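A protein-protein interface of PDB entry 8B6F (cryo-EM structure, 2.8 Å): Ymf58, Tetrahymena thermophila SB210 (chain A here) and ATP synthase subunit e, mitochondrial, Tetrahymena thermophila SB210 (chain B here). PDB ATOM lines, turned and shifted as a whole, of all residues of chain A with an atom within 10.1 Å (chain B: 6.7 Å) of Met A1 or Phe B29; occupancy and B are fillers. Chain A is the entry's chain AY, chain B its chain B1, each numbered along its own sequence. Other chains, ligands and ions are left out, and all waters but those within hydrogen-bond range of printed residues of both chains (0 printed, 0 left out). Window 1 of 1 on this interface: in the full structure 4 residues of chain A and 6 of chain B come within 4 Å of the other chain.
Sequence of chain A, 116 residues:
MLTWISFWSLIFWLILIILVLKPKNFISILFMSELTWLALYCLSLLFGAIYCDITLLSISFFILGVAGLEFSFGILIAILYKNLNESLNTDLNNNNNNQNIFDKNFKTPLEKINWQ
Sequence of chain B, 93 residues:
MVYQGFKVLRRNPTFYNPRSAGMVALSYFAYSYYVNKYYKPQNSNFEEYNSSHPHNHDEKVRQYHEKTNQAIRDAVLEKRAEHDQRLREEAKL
Met A1 touches Phe B29 (CE to CE1, 3.6 Å). CE of Met A1 touches OG of Ser B32, 3.1 Å away. CA of Ser B32 touches CD2 of Leu A2 (3.7 Å).
The side-chain hydroxyl (OG) of Ser B32 sits at hydrogen-bond distance from the backbone carbonyl oxygen (O) of Phe B29 (2.7 Å). The backbone carbonyl oxygen (O) of Tyr B28 is in hydrogen-bond range of the side-chain hydroxyl (OG) of Ser B32, at 3.2 Å. O of Ser B32 is in hydrogen-bond range of ND2 of Asn B36 (3.1 Å).
Hydrophobic or aromatic side chains of chain A that line the printed part of chain B: Met A1 and Leu A2. Printed residues of chain B that touch a printed residue of chain A: Tyr B28, Phe B29, Ser B32 and Asn B36. Among the printed residues, no Asp or Glu carboxylate lies within 4 Å of a Lys or Arg side-chain nitrogen of the other chain.
N of Met A1 sits close to OH of Tyr B28 (3.4 Å). The backbone carbonyl oxygen (O) of Met A1 sits at hydrogen-bond distance from the side-chain amide nitrogen (ND2) of Asn B36 (2.6 Å).
Met A1 touches just these residues of chain B: Tyr B28 (3.3 Å), Phe B29 (3.6 Å), Ser B32 (3.1 Å) and Asn B36 (2.6 Å). Printed residues of chain B within 4 Å of Leu A2: Ser B32. Ala B25 touches none of the printed residues of chain A. Of chain A, only Met A1 (3.3 Å) comes within 4 Å of Tyr B28. Printed residues of chain A within 4 Å of Phe B29: Met A1 (3.6 Å). Ala B30 touches none of the printed residues of chain A. Printed residues of chain A within 4 Å of Ser B32: Met A1 and Leu A2. Tyr B33 touches none of the printed residues of chain A. Printed residues of chain A within 4 Å of Asn B36: Met A1.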
ATOM      1  N   MET A   1       6.353  -9.208  15.944  1.00  0.00           N
ATOM      2  CA  MET A   1       6.557 -10.175  17.061  1.00  0.00           C
ATOM      3  C   MET A   1       5.844  -9.705  18.323  1.00  0.00           C
ATOM      4  O   MET A   1       5.348 -10.514  19.104  1.00  0.00           O
ATOM      5  CB  MET A   1       8.046 -10.361  17.347  1.00  0.00           C
ATOM      6  CG  MET A   1       8.829 -10.998  16.212  1.00  0.00           C
ATOM      7  SD  MET A   1       8.415 -12.733  15.941  1.00  0.00           S
ATOM      8  CE  MET A   1       8.952 -13.477  17.479  1.00  0.00           C
ATOM      9  N   LEU A   2       5.796  -8.391  18.513  1.00  0.00           N
ATOM     10  CA  LEU A   2       5.165  -7.775  19.670  1.00  0.00           C
ATOM     11  C   LEU A   2       3.911  -7.029  19.240  1.00  0.00           C
ATOM     12  O   LEU A   2       3.884  -6.399  18.179  1.00  0.00           O
ATOM     13  CB  LEU A   2       6.123  -6.802  20.364  1.00  0.00           C
ATOM     14  CG  LEU A   2       7.281  -7.403  21.160  1.00  0.00           C
ATOM     15  CD1 LEU A   2       8.245  -6.319  21.603  1.00  0.00           C
ATOM     16  CD2 LEU A   2       6.751  -8.157  22.366  1.00  0.00           C
ATOM     17  N   THR A   3       2.873  -7.102  20.067  1.00  0.00           N
ATOM     18  CA  THR A   3       1.695  -6.286  19.828  1.00  0.00           C
ATOM     19  C   THR A   3       2.085  -4.816  19.859  1.00  0.00           C
ATOM     20  O   THR A   3       3.018  -4.413  20.558  1.00  0.00           O
ATOM     21  CB  THR A   3       0.615  -6.563  20.877  1.00  0.00           C
ATOM     22  OG1 THR A   3       1.105  -6.212  22.177  1.00  0.00           O
ATOM     23  CG2 THR A   3       0.217  -8.027  20.869  1.00  0.00           C
ATOM     24  N   TRP A   4       1.364  -4.005  19.086  1.00  0.00           N
ATOM     25  CA  TRP A   4       1.729  -2.598  18.977  1.00  0.00           C
ATOM     26  C   TRP A   4       1.637  -1.902  20.326  1.00  0.00           C
ATOM     27  O   TRP A   4       2.462  -1.037  20.642  1.00  0.00           O
ATOM     28  CB  TRP A   4       0.843  -1.904  17.945  1.00  0.00           C
ATOM     29  CG  TRP A   4       1.165  -2.308  16.545  1.00  0.00           C
ATOM     30  CD1 TRP A   4       0.343  -2.947  15.667  1.00  0.00           C
ATOM     31  CD2 TRP A   4       2.408  -2.109  15.862  1.00  0.00           C
ATOM     32  NE1 TRP A   4       0.995  -3.155  14.477  1.00  0.00           N
ATOM     33  CE2 TRP A   4       2.265  -2.648  14.570  1.00  0.00           C
ATOM     34  CE3 TRP A   4       3.627  -1.522  16.217  1.00  0.00           C
ATOM     35  CZ2 TRP A   4       3.294  -2.620  13.633  1.00  0.00           C
ATOM     36  CZ3 TRP A   4       4.649  -1.496  15.286  1.00  0.00           C
ATOM     37  CH2 TRP A   4       4.474  -2.041  14.007  1.00  0.00           C
ATOM     38  N   ILE A   5       0.645  -2.265  21.140  1.00  0.00           N
ATOM     39  CA  ILE A   5       0.482  -1.613  22.436  1.00  0.00           C
ATOM     40  C   ILE A   5       1.725  -1.832  23.287  1.00  0.00           C
ATOM     41  O   ILE A   5       2.311  -0.884  23.821  1.00  0.00           O
ATOM     42  CB  ILE A   5      -0.783  -2.128  23.148  1.00  0.00           C
ATOM     43  CG1 ILE A   5      -2.060  -1.674  22.433  1.00  0.00           C
ATOM     44  CG2 ILE A   5      -0.826  -1.647  24.594  1.00  0.00           C
ATOM     45  CD1 ILE A   5      -2.374  -2.428  21.156  1.00  0.00           C
ATOM     46  N   SER A   6       2.140  -3.092  23.432  1.00  0.00           N
ATOM     47  CA  SER A   6       3.322  -3.384  24.236  1.00  0.00           C
ATOM     48  C   SER A   6       4.570  -2.780  23.609  1.00  0.00           C
ATOM     49  O   SER A   6       5.445  -2.270  24.318  1.00  0.00           O
ATOM     50  CB  SER A   6       3.483  -4.894  24.406  1.00  0.00           C
ATOM     51  OG  SER A   6       3.643  -5.538  23.156  1.00  0.00           O
ATOM     52  N   PHE A   7       4.677  -2.843  22.281  1.00  0.00           N
ATOM     53  CA  PHE A   7       5.856  -2.306  21.611  1.00  0.00           C
ATOM     54  C   PHE A   7       6.022  -0.821  21.898  1.00  0.00           C
ATOM     55  O   PHE A   7       7.100  -0.371  22.297  1.00  0.00           O
ATOM     56  CB  PHE A   7       5.762  -2.554  20.107  1.00  0.00           C
ATOM     57  CG  PHE A   7       6.896  -1.958  19.328  1.00  0.00           C
ATOM     58  CD1 PHE A   7       8.119  -2.602  19.264  1.00  0.00           C
ATOM     59  CD2 PHE A   7       6.741  -0.756  18.658  1.00  0.00           C
ATOM     60  CE1 PHE A   7       9.168  -2.060  18.550  1.00  0.00           C
ATOM     61  CE2 PHE A   7       7.786  -0.209  17.942  1.00  0.00           C
ATOM     62  CZ  PHE A   7       9.001  -0.862  17.889  1.00  0.00           C
ATOM     63  N   VAL B  24      21.113  -7.381  18.463  1.00  0.00           N
ATOM     64  CA  VAL B  24      19.849  -6.662  18.598  1.00  0.00           C
ATOM     65  C   VAL B  24      18.696  -7.533  18.117  1.00  0.00           C
ATOM     66  O   VAL B  24      17.655  -7.638  18.776  1.00  0.00           O
ATOM     67  CB  VAL B  24      19.908  -5.330  17.826  1.00  0.00           C
ATOM     68  CG1 VAL B  24      18.525  -4.714  17.691  1.00  0.00           C
ATOM     69  CG2 VAL B  24      20.836  -4.362  18.521  1.00  0.00           C
ATOM     70  N   ALA B  25      18.862  -8.165  16.954  1.00  0.00           N
ATOM     71  CA  ALA B  25      17.802  -9.016  16.424  1.00  0.00           C
ATOM     72  C   ALA B  25      17.504 -10.172  17.367  1.00  0.00           C
ATOM     73  O   ALA B  25      16.339 -10.491  17.625  1.00  0.00           O
ATOM     74  CB  ALA B  25      18.193  -9.541  15.043  1.00  0.00           C
ATOM     75  N   LEU B  26      18.550 -10.819  17.883  1.00  0.00           N
ATOM     76  CA  LEU B  26      18.353 -11.954  18.777  1.00  0.00           C
ATOM     77  C   LEU B  26      17.685 -11.528  20.078  1.00  0.00           C
ATOM     78  O   LEU B  26      16.788 -12.219  20.577  1.00  0.00           O
ATOM     79  CB  LEU B  26      19.695 -12.629  19.054  1.00  0.00           C
ATOM     80  CG  LEU B  26      19.636 -14.093  19.485  1.00  0.00           C
ATOM     81  CD1 LEU B  26      19.158 -14.972  18.337  1.00  0.00           C
ATOM     82  CD2 LEU B  26      20.994 -14.555  19.986  1.00  0.00           C
ATOM     83  N   SER B  27      18.106 -10.395  20.645  1.00  0.00           N
ATOM     84  CA  SER B  27      17.480  -9.907  21.870  1.00  0.00           C
ATOM     85  C   SER B  27      16.013  -9.573  21.643  1.00  0.00           C
ATOM     86  O   SER B  27      15.160  -9.883  22.481  1.00  0.00           O
ATOM     87  CB  SER B  27      18.228  -8.678  22.384  1.00  0.00           C
ATOM     88  OG  SER B  27      19.563  -8.998  22.728  1.00  0.00           O
ATOM     89  N   TYR B  28      15.703  -8.926  20.520  1.00  0.00           N
ATOM     90  CA  TYR B  28      14.316  -8.607  20.205  1.00  0.00           C
ATOM     91  C   TYR B  28      13.489  -9.876  20.065  1.00  0.00           C
ATOM     92  O   TYR B  28      12.377  -9.971  20.597  1.00  0.00           O
ATOM     93  CB  TYR B  28      14.263  -7.767  18.928  1.00  0.00           C
ATOM     94  CG  TYR B  28      12.900  -7.660  18.289  1.00  0.00           C
ATOM     95  CD1 TYR B  28      11.849  -7.032  18.943  1.00  0.00           C
ATOM     96  CD2 TYR B  28      12.673  -8.158  17.015  1.00  0.00           C
ATOM     97  CE1 TYR B  28      10.607  -6.922  18.353  1.00  0.00           C
ATOM     98  CE2 TYR B  28      11.436  -8.052  16.418  1.00  0.00           C
ATOM     99  CZ  TYR B  28      10.407  -7.433  17.091  1.00  0.00           C
ATOM    100  OH  TYR B  28       9.174  -7.327  16.495  1.00  0.00           O
ATOM    101  N   PHE B  29      14.022 -10.868  19.350  1.00  0.00           N
ATOM    102  CA  PHE B  29      13.307 -12.127  19.172  1.00  0.00           C
ATOM    103  C   PHE B  29      13.062 -12.809  20.512  1.00  0.00           C
ATOM    104  O   PHE B  29      11.949 -13.264  20.800  1.00  0.00           O
ATOM    105  CB  PHE B  29      14.102 -13.036  18.235  1.00  0.00           C
ATOM    106  CG  PHE B  29      13.407 -14.320  17.895  1.00  0.00           C
ATOM    107  CD1 PHE B  29      12.406 -14.345  16.939  1.00  0.00           C
ATOM    108  CD2 PHE B  29      13.772 -15.504  18.510  1.00  0.00           C
ATOM    109  CE1 PHE B  29      11.768 -15.526  16.616  1.00  0.00           C
ATOM    110  CE2 PHE B  29      13.139 -16.690  18.191  1.00  0.00           C
ATOM    111  CZ  PHE B  29      12.136 -16.700  17.242  1.00  0.00           C
ATOM    112  N   ALA B  30      14.099 -12.891  21.347  1.00  0.00           N
ATOM    113  CA  ALA B  30      13.967 -13.558  22.638  1.00  0.00           C
ATOM    114  C   ALA B  30      12.981 -12.833  23.545  1.00  0.00           C
ATOM    115  O   ALA B  30      12.160 -13.468  24.215  1.00  0.00           O
ATOM    116  CB  ALA B  30      15.333 -13.663  23.314  1.00  0.00           C
ATOM    117  N   TYR B  31      13.041 -11.500  23.578  1.00  0.00           N
ATOM    118  CA  TYR B  31      12.136 -10.748  24.440  1.00  0.00           C
ATOM    119  C   TYR B  31      10.693 -10.876  23.979  1.00  0.00           C
ATOM    120  O   TYR B  31       9.785 -11.019  24.804  1.00  0.00           O
ATOM    121  CB  TYR B  31      12.548  -9.279  24.489  1.00  0.00           C
ATOM    122  CG  TYR B  31      11.620  -8.440  25.334  1.00  0.00           C
ATOM    123  CD1 TYR B  31      11.689  -8.479  26.720  1.00  0.00           C
ATOM    124  CD2 TYR B  31      10.671  -7.617  24.747  1.00  0.00           C
ATOM    125  CE1 TYR B  31      10.839  -7.719  27.497  1.00  0.00           C
ATOM    126  CE2 TYR B  31       9.818  -6.855  25.514  1.00  0.00           C
ATOM    127  CZ  TYR B  31       9.908  -6.908  26.889  1.00  0.00           C
ATOM    128  OH  TYR B  31       9.059  -6.149  27.658  1.00  0.00           O
ATOM    129  N   SER B  32      10.456 -10.822  22.669  1.00  0.00           N
ATOM    130  CA  SER B  32       9.099 -11.010  22.175  1.00  0.00           C
ATOM    131  C   SER B  32       8.589 -12.396  22.536  1.00  0.00           C
ATOM    132  O   SER B  32       7.443 -12.549  22.975  1.00  0.00           O
ATOM    133  CB  SER B  32       9.053 -10.792  20.664  1.00  0.00           C
ATOM    134  OG  SER B  32       9.803 -11.785  19.987  1.00  0.00           O
ATOM    135  N   TYR B  33       9.421 -13.420  22.350  1.00  0.00           N
ATOM    136  CA  TYR B  33       9.025 -14.770  22.732  1.00  0.00           C
ATOM    137  C   TYR B  33       8.678 -14.829  24.212  1.00  0.00           C
ATOM    138  O   TYR B  33       7.617 -15.334  24.596  1.00  0.00           O
ATOM    139  CB  TYR B  33      10.141 -15.762  22.402  1.00  0.00           C
ATOM    140  CG  TYR B  33       9.755 -16.777  21.354  1.00  0.00           C
ATOM    141  CD1 TYR B  33       9.848 -16.478  20.002  1.00  0.00           C
ATOM    142  CD2 TYR B  33       9.300 -18.036  21.717  1.00  0.00           C
ATOM    143  CE1 TYR B  33       9.495 -17.402  19.042  1.00  0.00           C
ATOM    144  CE2 TYR B  33       8.944 -18.967  20.763  1.00  0.00           C
ATOM    145  CZ  TYR B  33       9.044 -18.643  19.428  1.00  0.00           C
ATOM    146  OH  TYR B  33       8.694 -19.568  18.475  1.00  0.00           O
ATOM    147  N   TYR B  34       9.571 -14.322  25.062  1.00  0.00           N
ATOM    148  CA  TYR B  34       9.334 -14.358  26.500  1.00  0.00           C
ATOM    149  C   TYR B  34       8.023 -13.670  26.854  1.00  0.00           C
ATOM    150  O   TYR B  34       7.168 -14.251  27.533  1.00  0.00           O
ATOM    151  CB  TYR B  34      10.512 -13.705  27.225  1.00  0.00           C
ATOM    152  CG  TYR B  34      10.218 -13.243  28.632  1.00  0.00           C
ATOM    153  CD1 TYR B  34      10.274 -14.128  29.700  1.00  0.00           C
ATOM    154  CD2 TYR B  34       9.910 -11.918  28.896  1.00  0.00           C
ATOM    155  CE1 TYR B  34      10.016 -13.708  30.990  1.00  0.00           C
ATOM    156  CE2 TYR B  34       9.650 -11.487  30.182  1.00  0.00           C
ATOM    157  CZ  TYR B  34       9.704 -12.386  31.225  1.00  0.00           C
ATOM    158  OH  TYR B  34       9.446 -11.960  32.505  1.00  0.00           O
ATOM    159  N   ASN B  36       5.276 -12.699  25.005  1.00  0.00           N
ATOM    160  CA  ASN B  36       4.044 -13.267  24.469  1.00  0.00           C
ATOM    161  C   ASN B  36       3.743 -14.632  25.075  1.00  0.00           C
ATOM    162  O   ASN B  36       2.596 -14.919  25.433  1.00  0.00           O
ATOM    163  CB  ASN B  36       4.140 -13.379  22.948  1.00  0.00           C
ATOM    164  CG  ASN B  36       4.153 -12.030  22.261  1.00  0.00           C
ATOM    165  OD1 ASN B  36       3.440 -11.112  22.659  1.00  0.00           O
ATOM    166  ND2 ASN B  36       4.969 -11.905  21.222  1.00  0.00           N
ATOM    167  N   LYS B  37       4.756 -15.492  25.184  1.00  0.00           N
ATOM    168  CA  LYS B  37       4.494 -16.870  25.586  1.00  0.00           C
ATOM    169  C   LYS B  37       4.277 -17.010  27.086  1.00  0.00           C
ATOM    170  O   LYS B  37       3.437 -17.807  27.516  1.00  0.00           O
ATOM    171  CB  LYS B  37       5.642 -17.772  25.130  1.00  0.00           C
ATOM    172  CG  LYS B  37       5.853 -17.790  23.623  1.00  0.00           C
ATOM    173  CD  LYS B  37       4.636 -18.345  22.896  1.00  0.00           C
ATOM    174  CE  LYS B  37       4.857 -18.390  21.396  1.00  0.00           C
ATOM    175  NZ  LYS B  37       5.040 -17.035  20.818  1.00  0.00           N
